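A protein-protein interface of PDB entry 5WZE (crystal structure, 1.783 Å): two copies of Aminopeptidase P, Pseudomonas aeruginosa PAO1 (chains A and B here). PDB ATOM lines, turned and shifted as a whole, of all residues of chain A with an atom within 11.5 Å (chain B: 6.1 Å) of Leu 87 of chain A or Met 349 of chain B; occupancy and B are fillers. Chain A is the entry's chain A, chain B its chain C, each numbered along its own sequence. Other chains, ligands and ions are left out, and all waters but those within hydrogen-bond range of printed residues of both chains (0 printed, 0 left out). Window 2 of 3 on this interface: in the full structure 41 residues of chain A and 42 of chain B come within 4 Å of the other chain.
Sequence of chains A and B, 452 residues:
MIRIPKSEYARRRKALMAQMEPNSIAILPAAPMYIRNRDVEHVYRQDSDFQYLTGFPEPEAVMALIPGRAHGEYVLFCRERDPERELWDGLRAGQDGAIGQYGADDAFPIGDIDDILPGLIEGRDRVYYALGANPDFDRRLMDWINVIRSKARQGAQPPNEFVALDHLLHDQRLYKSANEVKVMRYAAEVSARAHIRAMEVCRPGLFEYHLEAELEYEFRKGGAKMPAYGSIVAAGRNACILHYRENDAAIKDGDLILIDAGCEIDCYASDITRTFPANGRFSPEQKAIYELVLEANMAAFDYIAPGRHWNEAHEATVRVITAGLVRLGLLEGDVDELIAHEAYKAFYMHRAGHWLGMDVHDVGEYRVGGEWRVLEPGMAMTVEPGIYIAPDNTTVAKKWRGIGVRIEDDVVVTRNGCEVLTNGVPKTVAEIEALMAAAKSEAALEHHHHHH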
ATOM      1  N   ARG A  79       7.242 -16.602 -34.113  1.00  0.00           N
ATOM      2  CA  ARG A  79       7.067 -17.859 -33.391  1.00  0.00           C
ATOM      3  C   ARG A  79       7.059 -19.045 -34.346  1.00  0.00           C
ATOM      4  O   ARG A  79       6.470 -18.987 -35.425  1.00  0.00           O
ATOM      5  CB  ARG A  79       5.759 -17.848 -32.611  1.00  0.00           C
ATOM      6  CG  ARG A  79       5.698 -16.904 -31.450  1.00  0.00           C
ATOM      7  CD  ARG A  79       4.257 -16.635 -31.102  1.00  0.00           C
ATOM      8  NE  ARG A  79       4.097 -16.170 -29.735  1.00  0.00           N
ATOM      9  CZ  ARG A  79       2.927 -15.891 -29.178  1.00  0.00           C
ATOM     10  NH1 ARG A  79       1.814 -16.025 -29.876  1.00  0.00           N
ATOM     11  NH2 ARG A  79       2.871 -15.479 -27.925  1.00  0.00           N
ATOM     12  N   GLU A  80       7.694 -20.137 -33.934  1.00  0.00           N
ATOM     13  CA  GLU A  80       7.747 -21.327 -34.765  1.00  0.00           C
ATOM     14  C   GLU A  80       6.573 -22.252 -34.470  1.00  0.00           C
ATOM     15  O   GLU A  80       6.007 -22.253 -33.373  1.00  0.00           O
ATOM     16  CB  GLU A  80       9.076 -22.068 -34.578  1.00  0.00           C
ATOM     17  CG  GLU A  80       9.418 -22.451 -33.158  1.00  0.00           C
ATOM     18  CD  GLU A  80      10.800 -23.094 -33.040  1.00  0.00           C
ATOM     19  OE1 GLU A  80      11.357 -23.541 -34.070  1.00  0.00           O
ATOM     20  OE2 GLU A  80      11.332 -23.145 -31.914  1.00  0.00           O
ATOM     21  N   ARG A  81       6.204 -23.022 -35.486  1.00  0.00           N
ATOM     22  CA  ARG A  81       5.123 -23.984 -35.369  1.00  0.00           C
ATOM     23  C   ARG A  81       5.414 -24.954 -34.235  1.00  0.00           C
ATOM     24  O   ARG A  81       6.553 -25.378 -34.037  1.00  0.00           O
ATOM     25  CB  ARG A  81       4.956 -24.691 -36.714  1.00  0.00           C
ATOM     26  CG  ARG A  81       4.220 -25.982 -36.704  1.00  0.00           C
ATOM     27  CD  ARG A  81       4.518 -26.702 -38.016  1.00  0.00           C
ATOM     28  NE  ARG A  81       3.835 -27.980 -38.140  1.00  0.00           N
ATOM     29  CZ  ARG A  81       4.163 -28.910 -39.030  1.00  0.00           C
ATOM     30  NH1 ARG A  81       5.169 -28.703 -39.869  1.00  0.00           N
ATOM     31  NH2 ARG A  81       3.491 -30.049 -39.082  1.00  0.00           N
ATOM     32  N   ASP A  82       4.384 -25.246 -33.440  1.00  0.00           N
ATOM     33  CA  ASP A  82       4.553 -25.983 -32.192  1.00  0.00           C
ATOM     34  C   ASP A  82       3.210 -26.583 -31.848  1.00  0.00           C
ATOM     35  O   ASP A  82       2.335 -25.902 -31.293  1.00  0.00           O
ATOM     36  CB  ASP A  82       5.060 -25.085 -31.071  1.00  0.00           C
ATOM     37  CG  ASP A  82       5.432 -25.860 -29.829  1.00  0.00           C
ATOM     38  OD1 ASP A  82       5.675 -27.071 -29.940  1.00  0.00           O
ATOM     39  OD2 ASP A  82       5.497 -25.271 -28.736  1.00  0.00           O
ATOM     40  N   PRO A  83       3.012 -27.828 -32.146  1.00  0.00           N
ATOM     41  CA  PRO A  83       1.694 -28.425 -31.952  1.00  0.00           C
ATOM     42  C   PRO A  83       1.108 -28.366 -30.571  1.00  0.00           C
ATOM     43  O   PRO A  83      -0.061 -28.052 -30.483  1.00  0.00           O
ATOM     44  CB  PRO A  83       1.925 -29.862 -32.355  1.00  0.00           C
ATOM     45  CG  PRO A  83       2.963 -29.748 -33.390  1.00  0.00           C
ATOM     46  CD  PRO A  83       3.875 -28.640 -32.998  1.00  0.00           C
ATOM     47  N   GLU A  84       1.868 -28.615 -29.527  1.00  0.00           N
ATOM     48  CA  GLU A  84       1.286 -28.577 -28.221  1.00  0.00           C
ATOM     49  C   GLU A  84       0.779 -27.186 -27.923  1.00  0.00           C
ATOM     50  O   GLU A  84      -0.371 -27.019 -27.520  1.00  0.00           O
ATOM     51  CB  GLU A  84       2.279 -29.074 -27.172  1.00  0.00           C
ATOM     52  CG  GLU A  84       1.895 -28.876 -25.719  1.00  0.00           C
ATOM     53  CD  GLU A  84       2.447 -29.972 -24.807  1.00  0.00           C
ATOM     54  OE1 GLU A  84       1.653 -30.569 -24.062  1.00  0.00           O
ATOM     55  OE2 GLU A  84       3.661 -30.255 -24.844  1.00  0.00           O
ATOM     56  N   ARG A  85       1.583 -26.173 -28.192  1.00  0.00           N
ATOM     57  CA  ARG A  85       1.146 -24.822 -27.906  1.00  0.00           C
ATOM     58  C   ARG A  85      -0.028 -24.339 -28.719  1.00  0.00           C
ATOM     59  O   ARG A  85      -0.838 -23.567 -28.256  1.00  0.00           O
ATOM     60  CB  ARG A  85       2.286 -23.835 -27.923  1.00  0.00           C
ATOM     61  CG  ARG A  85       3.047 -23.836 -26.641  1.00  0.00           C
ATOM     62  CD  ARG A  85       2.307 -23.137 -25.531  1.00  0.00           C
ATOM     63  NE  ARG A  85       3.143 -23.245 -24.360  1.00  0.00           N
ATOM     64  CZ  ARG A  85       2.948 -24.113 -23.383  1.00  0.00           C
ATOM     65  NH1 ARG A  85       1.905 -24.921 -23.410  1.00  0.00           N
ATOM     66  NH2 ARG A  85       3.801 -24.155 -22.370  1.00  0.00           N
ATOM     67  N   GLU A  86      -0.062 -24.752 -29.958  1.00  0.00           N
ATOM     68  CA  GLU A  86      -1.147 -24.370 -30.816  1.00  0.00           C
ATOM     69  C   GLU A  86      -2.448 -24.973 -30.320  1.00  0.00           C
ATOM     70  O   GLU A  86      -3.475 -24.353 -30.470  1.00  0.00           O
ATOM     71  CB  GLU A  86      -0.836 -24.586 -32.293  1.00  0.00           C
ATOM     72  CG  GLU A  86       0.150 -23.536 -32.791  1.00  0.00           C
ATOM     73  CD  GLU A  86       0.551 -23.660 -34.240  1.00  0.00           C
ATOM     74  OE1 GLU A  86       1.682 -24.057 -34.495  1.00  0.00           O
ATOM     75  OE2 GLU A  86      -0.231 -23.344 -35.129  1.00  0.00           O
ATOM     76  N   LEU A  87      -2.396 -26.169 -29.728  1.00  0.00           N
ATOM     77  CA  LEU A  87      -3.619 -26.795 -29.248  1.00  0.00           C
ATOM     78  C   LEU A  87      -4.324 -25.881 -28.260  1.00  0.00           C
ATOM     79  O   LEU A  87      -5.546 -25.720 -28.315  1.00  0.00           O
ATOM     80  CB  LEU A  87      -3.321 -28.150 -28.620  1.00  0.00           C
ATOM     81  CG  LEU A  87      -4.613 -28.777 -28.108  1.00  0.00           C
ATOM     82  CD1 LEU A  87      -5.123 -29.715 -29.169  1.00  0.00           C
ATOM     83  CD2 LEU A  87      -4.296 -29.473 -26.820  1.00  0.00           C
ATOM     84  N   TRP A  88      -3.558 -25.223 -27.414  1.00  0.00           N
ATOM     85  CA  TRP A  88      -4.172 -24.295 -26.512  1.00  0.00           C
ATOM     86  C   TRP A  88      -4.335 -22.890 -27.037  1.00  0.00           C
ATOM     87  O   TRP A  88      -5.410 -22.335 -27.055  1.00  0.00           O
ATOM     88  CB  TRP A  88      -3.291 -24.178 -25.290  1.00  0.00           C
ATOM     89  CG  TRP A  88      -3.255 -25.392 -24.506  1.00  0.00           C
ATOM     90  CD1 TRP A  88      -2.619 -26.527 -24.806  1.00  0.00           C
ATOM     91  CD2 TRP A  88      -3.923 -25.613 -23.267  1.00  0.00           C
ATOM     92  NE1 TRP A  88      -2.830 -27.454 -23.843  1.00  0.00           N
ATOM     93  CE2 TRP A  88      -3.628 -26.911 -22.879  1.00  0.00           C
ATOM     94  CE3 TRP A  88      -4.723 -24.824 -22.445  1.00  0.00           C
ATOM     95  CZ2 TRP A  88      -4.108 -27.456 -21.713  1.00  0.00           C
ATOM     96  CZ3 TRP A  88      -5.203 -25.365 -21.283  1.00  0.00           C
ATOM     97  CH2 TRP A  88      -4.892 -26.667 -20.928  1.00  0.00           C
ATOM     98  N   ASP A  89      -3.219 -22.327 -27.459  1.00  0.00           N
ATOM     99  CA  ASP A  89      -3.124 -20.964 -27.927  1.00  0.00           C
ATOM    100  C   ASP A  89      -3.752 -20.431 -29.178  1.00  0.00           C
ATOM    101  O   ASP A  89      -4.269 -19.332 -29.154  1.00  0.00           O
ATOM    102  CB  ASP A  89      -1.675 -20.578 -27.928  1.00  0.00           C
ATOM    103  CG  ASP A  89      -1.168 -20.430 -26.560  1.00  0.00           C
ATOM    104  OD1 ASP A  89      -1.766 -19.615 -25.853  1.00  0.00           O
ATOM    105  OD2 ASP A  89      -0.211 -21.122 -26.185  1.00  0.00           O
ATOM    106  N   GLY A  90      -3.686 -21.160 -30.259  1.00  0.00           N
ATOM    107  CA  GLY A  90      -4.230 -20.674 -31.484  1.00  0.00           C
ATOM    108  C   GLY A  90      -3.189 -21.019 -32.465  1.00  0.00           C
ATOM    109  O   GLY A  90      -2.086 -21.282 -32.082  1.00  0.00           O
ATOM    110  N   LEU A  91      -3.547 -21.037 -33.724  1.00  0.00           N
ATOM    111  CA  LEU A  91      -2.608 -21.398 -34.729  1.00  0.00           C
ATOM    112  C   LEU A  91      -1.584 -20.307 -35.009  1.00  0.00           C
ATOM    113  O   LEU A  91      -1.913 -19.141 -34.921  1.00  0.00           O
ATOM    114  CB  LEU A  91      -3.333 -21.811 -35.971  1.00  0.00           C
ATOM    115  CG  LEU A  91      -4.358 -22.927 -35.777  1.00  0.00           C
ATOM    116  CD1 LEU A  91      -4.861 -23.325 -37.151  1.00  0.00           C
ATOM    117  CD2 LEU A  91      -3.710 -24.125 -35.112  1.00  0.00           C
ATOM    118  N   ARG A  92      -0.364 -20.711 -35.346  1.00  0.00           N
ATOM    119  CA  ARG A  92       0.712 -19.776 -35.619  1.00  0.00           C
ATOM    120  C   ARG A  92       1.071 -19.849 -37.090  1.00  0.00           C
ATOM    121  O   ARG A  92       1.009 -20.908 -37.706  1.00  0.00           O
ATOM    122  CB  ARG A  92       1.959 -20.085 -34.794  1.00  0.00           C
ATOM    123  CG  ARG A  92       1.761 -19.913 -33.319  1.00  0.00           C
ATOM    124  CD  ARG A  92       2.965 -20.391 -32.569  1.00  0.00           C
ATOM    125  NE  ARG A  92       2.830 -20.167 -31.139  1.00  0.00           N
ATOM    126  CZ  ARG A  92       3.775 -20.455 -30.250  1.00  0.00           C
ATOM    127  NH1 ARG A  92       4.920 -20.977 -30.651  1.00  0.00           N
ATOM    128  NH2 ARG A  92       3.575 -20.227 -28.962  1.00  0.00           N
ATOM    129  N   CYS B 240     -11.631 -27.203 -31.536  1.00  0.00           N
ATOM    130  CA  CYS B 240     -10.571 -28.043 -31.006  1.00  0.00           C
ATOM    131  C   CYS B 240      -9.364 -27.242 -30.518  1.00  0.00           C
ATOM    132  O   CYS B 240      -8.423 -27.831 -29.989  1.00  0.00           O
ATOM    133  CB  CYS B 240     -10.157 -29.073 -32.068  1.00  0.00           C
ATOM    134  SG  CYS B 240     -11.521 -30.139 -32.648  1.00  0.00           S
ATOM    135  N   ILE B 241      -9.370 -25.922 -30.650  1.00  0.00           N
ATOM    136  CA  ILE B 241      -8.303 -25.084 -30.117  1.00  0.00           C
ATOM    137  C   ILE B 241      -8.811 -24.488 -28.818  1.00  0.00           C
ATOM    138  O   ILE B 241      -9.808 -23.763 -28.824  1.00  0.00           O
ATOM    139  CB  ILE B 241      -7.901 -23.978 -31.101  1.00  0.00           C
ATOM    140  CG1 ILE B 241      -7.238 -24.551 -32.338  1.00  0.00           C
ATOM    141  CG2 ILE B 241      -6.935 -22.986 -30.440  1.00  0.00           C
ATOM    142  CD1 ILE B 241      -8.166 -25.112 -33.369  1.00  0.00           C
ATOM    143  N   LEU B 242      -8.184 -24.810 -27.705  1.00  0.00           N
ATOM    144  CA  LEU B 242      -8.695 -24.380 -26.409  1.00  0.00           C
ATOM    145  C   LEU B 242      -8.802 -22.895 -26.163  1.00  0.00           C
ATOM    146  O   LEU B 242      -9.721 -22.430 -25.576  1.00  0.00           O
ATOM    147  CB  LEU B 242      -7.893 -25.013 -25.281  1.00  0.00           C
ATOM    148  CG  LEU B 242      -7.741 -26.504 -25.295  1.00  0.00           C
ATOM    149  CD1 LEU B 242      -7.181 -27.065 -24.017  1.00  0.00           C
ATOM    150  CD2 LEU B 242      -9.072 -27.102 -25.604  1.00  0.00           C
ATOM    151  N   HIS B 243      -7.807 -22.168 -26.599  1.00  0.00           N
ATOM    152  CA  HIS B 243      -7.834 -20.744 -26.410  1.00  0.00           C
ATOM    153  C   HIS B 243      -7.938 -20.026 -27.756  1.00  0.00           C
ATOM    154  O   HIS B 243      -7.189 -19.126 -28.020  1.00  0.00           O
ATOM    155  CB  HIS B 243      -6.620 -20.255 -25.609  1.00  0.00           C
ATOM    156  CG  HIS B 243      -6.845 -20.174 -24.128  1.00  0.00           C
ATOM    157  ND1 HIS B 243      -6.523 -21.200 -23.269  1.00  0.00           N
ATOM    158  CD2 HIS B 243      -7.287 -19.164 -23.345  1.00  0.00           C
ATOM    159  CE1 HIS B 243      -6.796 -20.842 -22.029  1.00  0.00           C
ATOM    160  NE2 HIS B 243      -7.254 -19.607 -22.045  1.00  0.00           N
ATOM    161  N   TYR B 344      -6.762 -40.926 -22.289  1.00  0.00           N
ATOM    162  CA  TYR B 344      -7.853 -40.004 -22.573  1.00  0.00           C
ATOM    163  C   TYR B 344      -7.356 -38.611 -22.923  1.00  0.00           C
ATOM    164  O   TYR B 344      -8.117 -37.816 -23.483  1.00  0.00           O
ATOM    165  CB  TYR B 344      -8.800 -39.907 -21.377  1.00  0.00           C
ATOM    166  CG  TYR B 344      -8.111 -39.423 -20.133  1.00  0.00           C
ATOM    167  CD1 TYR B 344      -7.993 -38.063 -19.855  1.00  0.00           C
ATOM    168  CD2 TYR B 344      -7.553 -40.320 -19.250  1.00  0.00           C
ATOM    169  CE1 TYR B 344      -7.348 -37.621 -18.722  1.00  0.00           C
ATOM    170  CE2 TYR B 344      -6.902 -39.892 -18.119  1.00  0.00           C
ATOM    171  CZ  TYR B 344      -6.794 -38.547 -17.858  1.00  0.00           C
ATOM    172  OH  TYR B 344      -6.143 -38.147 -16.723  1.00  0.00           O
ATOM    173  N   LYS B 345      -6.111 -38.287 -22.581  1.00  0.00           N
ATOM    174  CA  LYS B 345      -5.625 -36.940 -22.830  1.00  0.00           C
ATOM    175  C   LYS B 345      -5.499 -36.638 -24.311  1.00  0.00           C
ATOM    176  O   LYS B 345      -5.422 -35.469 -24.682  1.00  0.00           O
ATOM    177  CB  LYS B 345      -4.299 -36.719 -22.104  1.00  0.00           C
ATOM    178  CG  LYS B 345      -4.486 -36.605 -20.595  1.00  0.00           C
ATOM    179  CD  LYS B 345      -3.325 -35.917 -19.911  1.00  0.00           C
ATOM    180  CE  LYS B 345      -3.604 -35.708 -18.437  1.00  0.00           C
ATOM    181  NZ  LYS B 345      -2.482 -34.983 -17.780  1.00  0.00           N
ATOM    182  N   ALA B 346      -5.543 -37.652 -25.169  1.00  0.00           N
ATOM    183  CA  ALA B 346      -5.662 -37.373 -26.590  1.00  0.00           C
ATOM    184  C   ALA B 346      -6.963 -36.654 -26.919  1.00  0.00           C
ATOM    185  O   ALA B 346      -7.038 -35.978 -27.946  1.00  0.00           O
ATOM    186  CB  ALA B 346      -5.552 -38.662 -27.402  1.00  0.00           C
ATOM    187  N   PHE B 347      -7.973 -36.747 -26.055  1.00  0.00           N
ATOM    188  CA  PHE B 347      -9.258 -36.108 -26.301  1.00  0.00           C
ATOM    189  C   PHE B 347      -9.686 -35.118 -25.236  1.00  0.00           C
ATOM    190  O   PHE B 347     -10.502 -34.247 -25.537  1.00  0.00           O
ATOM    191  CB  PHE B 347     -10.364 -37.165 -26.449  1.00  0.00           C
ATOM    192  CG  PHE B 347     -10.036 -38.228 -27.436  1.00  0.00           C
ATOM    193  CD1 PHE B 347     -10.145 -37.989 -28.783  1.00  0.00           C
ATOM    194  CD2 PHE B 347      -9.588 -39.461 -27.016  1.00  0.00           C
ATOM    195  CE1 PHE B 347      -9.821 -38.963 -29.692  1.00  0.00           C
ATOM    196  CE2 PHE B 347      -9.276 -40.434 -27.921  1.00  0.00           C
ATOM    197  CZ  PHE B 347      -9.392 -40.186 -29.254  1.00  0.00           C
ATOM    198  N   TYR B 348      -9.160 -35.221 -24.014  1.00  0.00           N
ATOM    199  CA  TYR B 348      -9.553 -34.397 -22.866  1.00  0.00           C
ATOM    200  C   TYR B 348      -8.273 -34.067 -22.104  1.00  0.00           C
ATOM    201  O   TYR B 348      -7.867 -34.815 -21.213  1.00  0.00           O
ATOM    202  CB  TYR B 348     -10.546 -35.132 -21.999  1.00  0.00           C
ATOM    203  CG  TYR B 348     -10.992 -34.463 -20.724  1.00  0.00           C
ATOM    204  CD1 TYR B 348     -11.210 -33.103 -20.655  1.00  0.00           C
ATOM    205  CD2 TYR B 348     -11.256 -35.220 -19.600  1.00  0.00           C
ATOM    206  CE1 TYR B 348     -11.643 -32.518 -19.496  1.00  0.00           C
ATOM    207  CE2 TYR B 348     -11.698 -34.642 -18.435  1.00  0.00           C
ATOM    208  CZ  TYR B 348     -11.893 -33.290 -18.388  1.00  0.00           C
ATOM    209  OH  TYR B 348     -12.344 -32.718 -17.230  1.00  0.00           O
ATOM    210  N   MET B 349      -7.653 -32.946 -22.454  1.00  0.00           N
ATOM    211  CA  MET B 349      -6.287 -32.664 -22.037  1.00  0.00           C
ATOM    212  C   MET B 349      -6.171 -31.514 -21.041  1.00  0.00           C
ATOM    213  O   MET B 349      -5.057 -31.077 -20.753  1.00  0.00           O
ATOM    214  CB  MET B 349      -5.420 -32.383 -23.264  1.00  0.00           C
ATOM    215  CG  MET B 349      -5.765 -31.110 -24.010  1.00  0.00           C
ATOM    216  SD  MET B 349      -7.334 -31.166 -24.932  1.00  0.00           S
ATOM    217  CE  MET B 349      -7.096 -32.585 -25.974  1.00  0.00           C
ATOM    218  N   HIS B 350      -7.276 -31.029 -20.488  1.00  0.00           N
ATOM    219  CA  HIS B 350      -7.240 -29.990 -19.474  1.00  0.00           C
ATOM    220  C   HIS B 350      -8.017 -30.429 -18.243  1.00  0.00           C
ATOM    221  O   HIS B 350      -8.707 -31.447 -18.249  1.00  0.00           O
ATOM    222  CB  HIS B 350      -7.814 -28.677 -19.998  1.00  0.00           C
ATOM    223  CG  HIS B 350      -9.247 -28.775 -20.422  1.00  0.00           C
ATOM    224  ND1 HIS B 350     -10.292 -28.791 -19.526  1.00  0.00           N
ATOM    225  CD2 HIS B 350      -9.808 -28.830 -21.651  1.00  0.00           C
ATOM    226  CE1 HIS B 350     -11.431 -28.865 -20.185  1.00  0.00           C
ATOM    227  NE2 HIS B 350     -11.166 -28.893 -21.475  1.00  0.00           N
ATOM    228  N   ARG B 351      -7.923 -29.629 -17.187  1.00  0.00           N
ATOM    229  CA  ARG B 351      -8.563 -29.961 -15.931  1.00  0.00           C
ATOM    230  C   ARG B 351     -10.039 -29.590 -15.977  1.00  0.00           C
ATOM    231  O   ARG B 351     -10.484 -28.807 -16.814  1.00  0.00           O
ATOM    232  CB  ARG B 351      -7.879 -29.253 -14.762  1.00  0.00           C
ATOM    233  CG  ARG B 351      -6.452 -29.747 -14.440  1.00  0.00           C
ATOM    234  CD  ARG B 351      -6.454 -31.127 -13.792  1.00  0.00           C
ATOM    235  NE  ARG B 351      -5.253 -31.411 -13.004  1.00  0.00           N
ATOM    236  CZ  ARG B 351      -4.242 -32.180 -13.400  1.00  0.00           C
ATOM    237  NH1 ARG B 351      -4.260 -32.764 -14.590  1.00  0.00           N
ATOM    238  NH2 ARG B 351      -3.201 -32.366 -12.600  1.00  0.00           N
ATOM    239  N   GLY B 386     -14.636 -31.510 -21.281  1.00  0.00           N
ATOM    240  CA  GLY B 386     -14.774 -31.397 -22.723  1.00  0.00           C
ATOM    241  C   GLY B 386     -14.127 -32.561 -23.444  1.00  0.00           C
ATOM    242  O   GLY B 386     -13.385 -33.346 -22.857  1.00  0.00           O
ATOM    243  N   TYR B 388     -12.342 -33.210 -27.476  1.00  0.00           N
ATOM    244  CA  TYR B 388     -11.886 -32.526 -28.679  1.00  0.00           C
ATOM    245  C   TYR B 388     -11.172 -33.546 -29.551  1.00  0.00           C
ATOM    246  O   TYR B 388     -10.122 -34.063 -29.169  1.00  0.00           O
ATOM    247  CB  TYR B 388     -10.959 -31.358 -28.335  1.00  0.00           C
ATOM    248  CG  TYR B 388     -11.422 -30.558 -27.151  1.00  0.00           C
ATOM    249  CD1 TYR B 388     -11.073 -30.924 -25.864  1.00  0.00           C
ATOM    250  CD2 TYR B 388     -12.222 -29.437 -27.317  1.00  0.00           C
ATOM    251  CE1 TYR B 388     -11.503 -30.206 -24.775  1.00  0.00           C
ATOM    252  CE2 TYR B 388     -12.662 -28.703 -26.224  1.00  0.00           C
ATOM    253  CZ  TYR B 388     -12.298 -29.090 -24.960  1.00  0.00           C
ATOM    254  OH  TYR B 388     -12.723 -28.382 -23.880  1.00  0.00           O
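N of Leu 242 of chain B lies within hydrogen-bond range of O of Leu 87 of chain A (2.9 Å).
The backbone carbonyl oxygen of Trp 88 of chain A is in hydrogen-bond range of the backbone NH of His 243 of chain B.
O of Asp 89 of chain A sits close to O of His 243 of chain B, 3.1 Å away.
OE1 of Glu 86 of chain A lies within hydrogen-bond range of N of Asp 82 of chain A, 3.1 Å away.
The backbone NH of Arg 92 of chain A sits at hydrogen-bond distance from the side-chain carboxylate of Glu 86 of chain A.
OH of Tyr 388 of chain B is in hydrogen-bond range of NE2 of His 350 of chain B (2.9 Å).
Ile 241 of chain B touches Glu 86 of chain A.
Cys 240 of chain B touches Leu 87 of chain A.
O of Leu 87 of chain A touches CA of Ile 241 of chain B, at 3.4 Å.
Met 349 of chain B touches Leu 87 of chain A.
O of Trp 88 of chain A touches CG2 of Ile 241 of chain B, 3.8 Å away.
Trp 88 of chain A touches Leu 242 of chain B (O to C, 3.6 Å).
CZ2 of Trp 88 of chain A touches O of Met 349 of chain B, 3.9 Å away.
His 350 of chain B touches Trp 88 of chain A (CB to CH2, 3.7 Å).
Gly 90 of chain A touches Ile 241 of chain B.
Printed residues of chain B within 4 Å of Glu 86 of chain A: Ile 241 (3.7 Å).
Leu 87 of chain A touches just these residues of chain B: Cys 240, Ile 241, Leu 242 and Met 349.
Of the printed residues of chain B, Asp 89 of chain A touches His 243 (3.1 Å).
Printed residues of chain B within 4 Å of Gly 90 of chain A: Ile 241 (3.7 Å).
Cys 240 of chain B touches just one residue of chain A: Leu 87 (3.9 Å).
Leu 242 of chain B touches just these residues of chain A: Leu 87 and Trp 88.
Of the printed residues of chain A, His 243 of chain B touches Trp 88 (2.4 Å) and Asp 89 (3.1 Å).
Tyr 348 of chain B touches none of the printed residues of chain A.
Printed residues of chain A within 4 Å of Met 349 of chain B: Leu 87 (3.6 Å) and Trp 88 (3.9 Å).
His 350 of chain B touches just one residue of chain A: Trp 88.
No residue of chain A comes within 4 Å of Gly 386 of chain B.
No residue of chain A comes within 4 Å of Tyr 388 of chain B.
The nearest printed residue of chain B that does not touch Glu 86 of chain A is Leu 242 of chain B (5.5 Å).
Of the 14 printed residues of chain B, 6 touch a printed residue of chain A.
Printed residues of chain B that touch a printed residue of chain A: Cys 240, Ile 241, Leu 242, His 243, Met 349 and His 350.
Hydrophobic or aromatic side chains of chain B that line the printed part of chain A: Ile 241, Leu 242, His 243, Met 349 and His 350.
Printed residues of chain A that touch a printed residue of chain B: Glu 86, Leu 87, Trp 88, Asp 89 and Gly 90.
Along chain A the printed residues that touch a printed residue of chain B span positions 86 to 90.
No position is printed for both chains.
Of the 12 pairs that touch across the chains among the printed residues, none has its exchanged pair printed and touching as well.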
